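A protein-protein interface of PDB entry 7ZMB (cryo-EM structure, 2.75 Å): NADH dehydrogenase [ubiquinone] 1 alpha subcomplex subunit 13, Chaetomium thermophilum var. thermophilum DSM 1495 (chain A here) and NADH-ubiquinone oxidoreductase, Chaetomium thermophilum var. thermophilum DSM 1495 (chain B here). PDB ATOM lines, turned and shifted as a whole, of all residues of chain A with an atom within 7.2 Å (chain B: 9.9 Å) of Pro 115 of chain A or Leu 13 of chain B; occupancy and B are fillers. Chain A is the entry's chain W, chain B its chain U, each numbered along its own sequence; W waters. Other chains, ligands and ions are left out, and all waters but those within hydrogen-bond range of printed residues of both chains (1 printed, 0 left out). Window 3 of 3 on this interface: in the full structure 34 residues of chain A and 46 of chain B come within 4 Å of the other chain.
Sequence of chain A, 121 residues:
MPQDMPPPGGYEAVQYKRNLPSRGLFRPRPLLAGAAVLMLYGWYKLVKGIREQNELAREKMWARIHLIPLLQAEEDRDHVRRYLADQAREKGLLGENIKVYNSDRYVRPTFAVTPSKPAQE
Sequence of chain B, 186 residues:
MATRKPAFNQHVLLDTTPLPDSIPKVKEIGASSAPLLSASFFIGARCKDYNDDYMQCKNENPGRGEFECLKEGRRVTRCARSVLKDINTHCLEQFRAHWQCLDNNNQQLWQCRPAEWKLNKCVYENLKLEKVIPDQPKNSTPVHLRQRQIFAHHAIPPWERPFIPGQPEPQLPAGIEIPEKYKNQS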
ATOM      1  N   ARG A  82     -31.571   2.424  -5.669  1.00  0.00           N
ATOM      2  CA  ARG A  82     -30.096   2.261  -5.623  1.00  0.00           C
ATOM      3  C   ARG A  82     -29.626   1.836  -4.243  1.00  0.00           C
ATOM      4  O   ARG A  82     -28.576   1.198  -4.172  1.00  0.00           O
ATOM      5  CB  ARG A  82     -29.391   3.514  -6.156  1.00  0.00           C
ATOM      6  CG  ARG A  82     -29.792   3.876  -7.579  1.00  0.00           C
ATOM      7  CD  ARG A  82     -29.074   5.047  -8.213  1.00  0.00           C
ATOM      8  NE  ARG A  82     -27.644   4.828  -8.337  1.00  0.00           N
ATOM      9  CZ  ARG A  82     -26.850   5.475  -9.179  1.00  0.00           C
ATOM     10  NH1 ARG A  82     -25.558   5.204  -9.206  1.00  0.00           N
ATOM     11  NH2 ARG A  82     -27.350   6.380  -9.998  1.00  0.00           N
ATOM     12  N   ALA A 112     -19.833   6.885  -3.152  1.00  0.00           N
ATOM     13  CA  ALA A 112     -20.362   5.779  -3.927  1.00  0.00           C
ATOM     14  C   ALA A 112     -19.212   4.945  -4.459  1.00  0.00           C
ATOM     15  O   ALA A 112     -18.142   5.465  -4.776  1.00  0.00           O
ATOM     16  CB  ALA A 112     -21.230   6.254  -5.092  1.00  0.00           C
ATOM     17  N   VAL A 113     -19.445   3.637  -4.542  1.00  0.00           N
ATOM     18  CA  VAL A 113     -18.519   2.757  -5.237  1.00  0.00           C
ATOM     19  C   VAL A 113     -18.669   2.955  -6.737  1.00  0.00           C
ATOM     20  O   VAL A 113     -19.784   2.931  -7.276  1.00  0.00           O
ATOM     21  CB  VAL A 113     -18.765   1.299  -4.836  1.00  0.00           C
ATOM     22  CG1 VAL A 113     -17.881   0.387  -5.638  1.00  0.00           C
ATOM     23  CG2 VAL A 113     -18.493   1.128  -3.368  1.00  0.00           C
ATOM     24  N   THR A 114     -17.554   3.168  -7.415  1.00  0.00           N
ATOM     25  CA  THR A 114     -17.512   3.323  -8.855  1.00  0.00           C
ATOM     26  C   THR A 114     -16.678   2.210  -9.470  1.00  0.00           C
ATOM     27  O   THR A 114     -15.812   1.630  -8.805  1.00  0.00           O
ATOM     28  CB  THR A 114     -16.914   4.681  -9.257  1.00  0.00           C
ATOM     29  OG1 THR A 114     -15.486   4.625  -9.167  1.00  0.00           O
ATOM     30  CG2 THR A 114     -17.425   5.789  -8.363  1.00  0.00           C
ATOM     31  N   PRO A 115     -16.914   1.878 -10.737  1.00  0.00           N
ATOM     32  CA  PRO A 115     -15.983   1.004 -11.448  1.00  0.00           C
ATOM     33  C   PRO A 115     -14.651   1.697 -11.675  1.00  0.00           C
ATOM     34  O   PRO A 115     -14.537   2.923 -11.631  1.00  0.00           O
ATOM     35  CB  PRO A 115     -16.701   0.721 -12.769  1.00  0.00           C
ATOM     36  CG  PRO A 115     -17.625   1.856 -12.937  1.00  0.00           C
ATOM     37  CD  PRO A 115     -18.081   2.218 -11.567  1.00  0.00           C
ATOM     38  N   SER A 116     -13.625   0.884 -11.914  1.00  0.00           N
ATOM     39  CA  SER A 116     -12.273   1.404 -12.049  1.00  0.00           C
ATOM     40  C   SER A 116     -12.045   2.153 -13.352  1.00  0.00           C
ATOM     41  O   SER A 116     -11.026   2.841 -13.474  1.00  0.00           O
ATOM     42  CB  SER A 116     -11.262   0.264 -11.935  1.00  0.00           C
ATOM     43  OG  SER A 116      -9.954   0.721 -12.227  1.00  0.00           O
ATOM     44  N   LYS A 117     -12.948   2.045 -14.318  1.00  0.00           N
ATOM     45  CA  LYS A 117     -12.783   2.688 -15.611  1.00  0.00           C
ATOM     46  C   LYS A 117     -14.111   3.281 -16.059  1.00  0.00           C
ATOM     47  O   LYS A 117     -15.174   2.734 -15.747  1.00  0.00           O
ATOM     48  CB  LYS A 117     -12.270   1.688 -16.662  1.00  0.00           C
ATOM     49  CG  LYS A 117     -11.781   2.308 -17.964  1.00  0.00           C
ATOM     50  CD  LYS A 117     -11.223   1.261 -18.914  1.00  0.00           C
ATOM     51  CE  LYS A 117      -9.752   0.988 -18.639  1.00  0.00           C
ATOM     52  NZ  LYS A 117      -9.088   0.310 -19.786  1.00  0.00           N
ATOM     53  N   PRO A 118     -14.131   4.465 -16.734  1.00  0.00           N
ATOM     54  CA  PRO A 118     -15.361   5.010 -17.332  1.00  0.00           C
ATOM     55  C   PRO A 118     -15.650   4.344 -18.689  1.00  0.00           C
ATOM     56  O   PRO A 118     -14.768   3.668 -19.203  1.00  0.00           O
ATOM     57  CB  PRO A 118     -15.089   6.508 -17.542  1.00  0.00           C
ATOM     58  CG  PRO A 118     -13.796   6.778 -16.815  1.00  0.00           C
ATOM     59  CD  PRO A 118     -13.050   5.465 -16.879  1.00  0.00           C
ATOM     60  N   ALA A 119     -16.845   4.547 -19.245  1.00  0.00           N
ATOM     61  CA  ALA A 119     -17.210   3.846 -20.498  1.00  0.00           C
ATOM     62  C   ALA A 119     -16.167   4.156 -21.578  1.00  0.00           C
ATOM     63  O   ALA A 119     -15.761   5.328 -21.693  1.00  0.00           O
ATOM     64  CB  ALA A 119     -18.599   4.242 -20.934  1.00  0.00           C
ATOM     65  N   MET B   1     -27.928  10.047  -3.162  1.00  0.00           N
ATOM     66  CA  MET B   1     -26.652  10.797  -3.123  1.00  0.00           C
ATOM     67  C   MET B   1     -26.885  12.175  -2.511  1.00  0.00           C
ATOM     68  O   MET B   1     -28.050  12.578  -2.438  1.00  0.00           O
ATOM     69  CB  MET B   1     -26.032  10.891  -4.514  1.00  0.00           C
ATOM     70  N   ASN B   9     -17.701  18.122 -10.888  1.00  0.00           N
ATOM     71  CA  ASN B   9     -18.284  16.853 -11.404  1.00  0.00           C
ATOM     72  C   ASN B   9     -17.900  16.624 -12.870  1.00  0.00           C
ATOM     73  O   ASN B   9     -18.416  17.327 -13.725  1.00  0.00           O
ATOM     74  CB  ASN B   9     -19.809  16.845 -11.269  1.00  0.00           C
ATOM     75  CG  ASN B   9     -20.486  18.103 -11.776  1.00  0.00           C
ATOM     76  OD1 ASN B   9     -20.095  19.212 -11.429  1.00  0.00           O
ATOM     77  ND2 ASN B   9     -21.518  17.940 -12.583  1.00  0.00           N
ATOM     78  N   GLN B  10     -17.001  15.686 -13.136  1.00  0.00           N
ATOM     79  CA  GLN B  10     -16.602  15.383 -14.534  1.00  0.00           C
ATOM     80  C   GLN B  10     -17.167  14.024 -14.947  1.00  0.00           C
ATOM     81  O   GLN B  10     -16.941  13.623 -16.095  1.00  0.00           O
ATOM     82  CB  GLN B  10     -15.077  15.432 -14.658  1.00  0.00           C
ATOM     83  CG  GLN B  10     -14.428  16.646 -14.005  1.00  0.00           C
ATOM     84  CD  GLN B  10     -14.610  17.930 -14.780  1.00  0.00           C
ATOM     85  OE1 GLN B  10     -15.714  18.292 -15.185  1.00  0.00           O
ATOM     86  NE2 GLN B  10     -13.519  18.649 -14.974  1.00  0.00           N
ATOM     87  N   HIS B  11     -17.914  13.364 -14.058  1.00  0.00           N
ATOM     88  CA  HIS B  11     -18.397  11.987 -14.340  1.00  0.00           C
ATOM     89  C   HIS B  11     -19.818  11.779 -13.839  1.00  0.00           C
ATOM     90  O   HIS B  11     -20.251  12.548 -12.968  1.00  0.00           O
ATOM     91  CB  HIS B  11     -17.457  10.947 -13.707  1.00  0.00           C
ATOM     92  CG  HIS B  11     -16.078  10.977 -14.267  1.00  0.00           C
ATOM     93  ND1 HIS B  11     -15.796  10.536 -15.541  1.00  0.00           N
ATOM     94  CD2 HIS B  11     -14.911  11.409 -13.744  1.00  0.00           C
ATOM     95  CE1 HIS B  11     -14.509  10.682 -15.780  1.00  0.00           C
ATOM     96  NE2 HIS B  11     -13.944  11.215 -14.691  1.00  0.00           N
ATOM     97  N   VAL B  12     -20.503  10.771 -14.374  1.00  0.00           N
ATOM     98  CA  VAL B  12     -21.890  10.431 -13.940  1.00  0.00           C
ATOM     99  C   VAL B  12     -21.918   8.930 -13.627  1.00  0.00           C
ATOM    100  O   VAL B  12     -21.234   8.172 -14.333  1.00  0.00           O
ATOM    101  CB  VAL B  12     -22.906  10.823 -15.032  1.00  0.00           C
ATOM    102  CG1 VAL B  12     -24.222  10.072 -14.907  1.00  0.00           C
ATOM    103  CG2 VAL B  12     -23.156  12.321 -15.066  1.00  0.00           C
ATOM    104  N   LEU B  13     -22.654   8.522 -12.590  1.00  0.00           N
ATOM    105  CA  LEU B  13     -22.752   7.090 -12.217  1.00  0.00           C
ATOM    106  C   LEU B  13     -24.194   6.595 -12.326  1.00  0.00           C
ATOM    107  O   LEU B  13     -25.076   7.256 -11.766  1.00  0.00           O
ATOM    108  CB  LEU B  13     -22.212   6.902 -10.798  1.00  0.00           C
ATOM    109  CG  LEU B  13     -22.105   5.462 -10.303  1.00  0.00           C
ATOM    110  CD1 LEU B  13     -21.158   4.653 -11.173  1.00  0.00           C
ATOM    111  CD2 LEU B  13     -21.642   5.437  -8.860  1.00  0.00           C
ATOM    112  N   LEU B  14     -24.407   5.485 -13.031  1.00  0.00           N
ATOM    113  CA  LEU B  14     -25.732   4.908 -13.209  1.00  0.00           C
ATOM    114  C   LEU B  14     -25.843   3.581 -12.468  1.00  0.00           C
ATOM    115  O   LEU B  14     -24.879   3.072 -11.896  1.00  0.00           O
ATOM    116  CB  LEU B  14     -26.063   4.719 -14.695  1.00  0.00           C
ATOM    117  CG  LEU B  14     -26.503   5.962 -15.478  1.00  0.00           C
ATOM    118  CD1 LEU B  14     -25.322   6.784 -15.916  1.00  0.00           C
ATOM    119  CD2 LEU B  14     -27.352   5.603 -16.660  1.00  0.00           C
ATOM    120  N   ASP B  15     -27.049   3.023 -12.477  1.00  0.00           N
ATOM    121  CA  ASP B  15     -27.335   1.782 -11.764  1.00  0.00           C
ATOM    122  C   ASP B  15     -28.418   1.022 -12.514  1.00  0.00           C
ATOM    123  O   ASP B  15     -29.600   1.352 -12.398  1.00  0.00           O
ATOM    124  CB  ASP B  15     -27.772   2.060 -10.328  1.00  0.00           C
ATOM    125  CG  ASP B  15     -27.517   0.883  -9.408  1.00  0.00           C
ATOM    126  OD1 ASP B  15     -26.463   0.230  -9.561  1.00  0.00           O
ATOM    127  OD2 ASP B  15     -28.364   0.615  -8.536  1.00  0.00           O
ATOM    128  N   THR B  16     -28.024  -0.009 -13.260  1.00  0.00           N
ATOM    129  CA  THR B  16     -28.970  -0.736 -14.098  1.00  0.00           C
ATOM    130  C   THR B  16     -29.901  -1.637 -13.296  1.00  0.00           C
ATOM    131  O   THR B  16     -30.811  -2.226 -13.882  1.00  0.00           O
ATOM    132  CB  THR B  16     -28.221  -1.566 -15.143  1.00  0.00           C
ATOM    133  OG1 THR B  16     -27.354  -2.493 -14.483  1.00  0.00           O
ATOM    134  CG2 THR B  16     -27.393  -0.673 -16.033  1.00  0.00           C
HETATM  135  O   HOH W   1     -28.835   5.229 -12.593  1.00  0.00           O
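Of the 9 printed residues of chain B, 3 touch a printed residue of chain A. Along chain B the printed residues that touch a printed residue of chain A span positions 13 to 15. Hydrophobic or aromatic side chains of chain A within 4 Å of the printed part of chain B: Ala 112 and Pro 115.
Of the printed residues of chain B, Arg 82 of chain A touches Leu 13, Leu 14 and Asp 15. Of the printed residues of chain B, Ala 112 of chain A touches Leu 13 (3.9 Å). Of the printed residues of chain B, Val 113 of chain A touches Leu 13. No residue of chain B comes within 4 Å of Thr 114 of chain A. Of chain B, only Leu 13 comes within 4 Å of Pro 115 of chain A. No residue of chain B comes within 4 Å of Ser 116 of chain A. His 11 of chain B touches none of the printed residues of chain A. Of chain A, only Arg 82, Ala 112, Val 113 and Pro 115 come within 4 Å of Leu 13 of chain B. Of the printed residues of chain A, Asp 15 of chain B touches Arg 82 (3.4 Å). The nearest residue of chain B that does not touch Pro 115 of chain A is Leu 14 of chain B (6.9 Å).
Water W1 lies within hydrogen-bond range of the backbone NH of Asp 15 of chain B (2.8 Å) and the guanidinium group of Arg 82 of chain A (3.2 Å).
NH1 of Arg 82 of chain A lies within hydrogen-bond range of O of Leu 14 of chain B (3.5 Å). The guanidinium group of Arg 82 of chain A sits at hydrogen-bond distance from the backbone carbonyl oxygen of Leu 13 of chain B (3.0 Å).
Among the printed residues, pairs that only touch across the chains: Arg 82 of chain A with Asp 15 of chain B (3.4 Å), Val 113 of chain A with Leu 13 of chain B (3.5 Å), Ala 112 of chain A with Leu 13 of chain B (3.9 Å) and Pro 115 of chain A with Leu 13 of chain B (3.9 Å).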
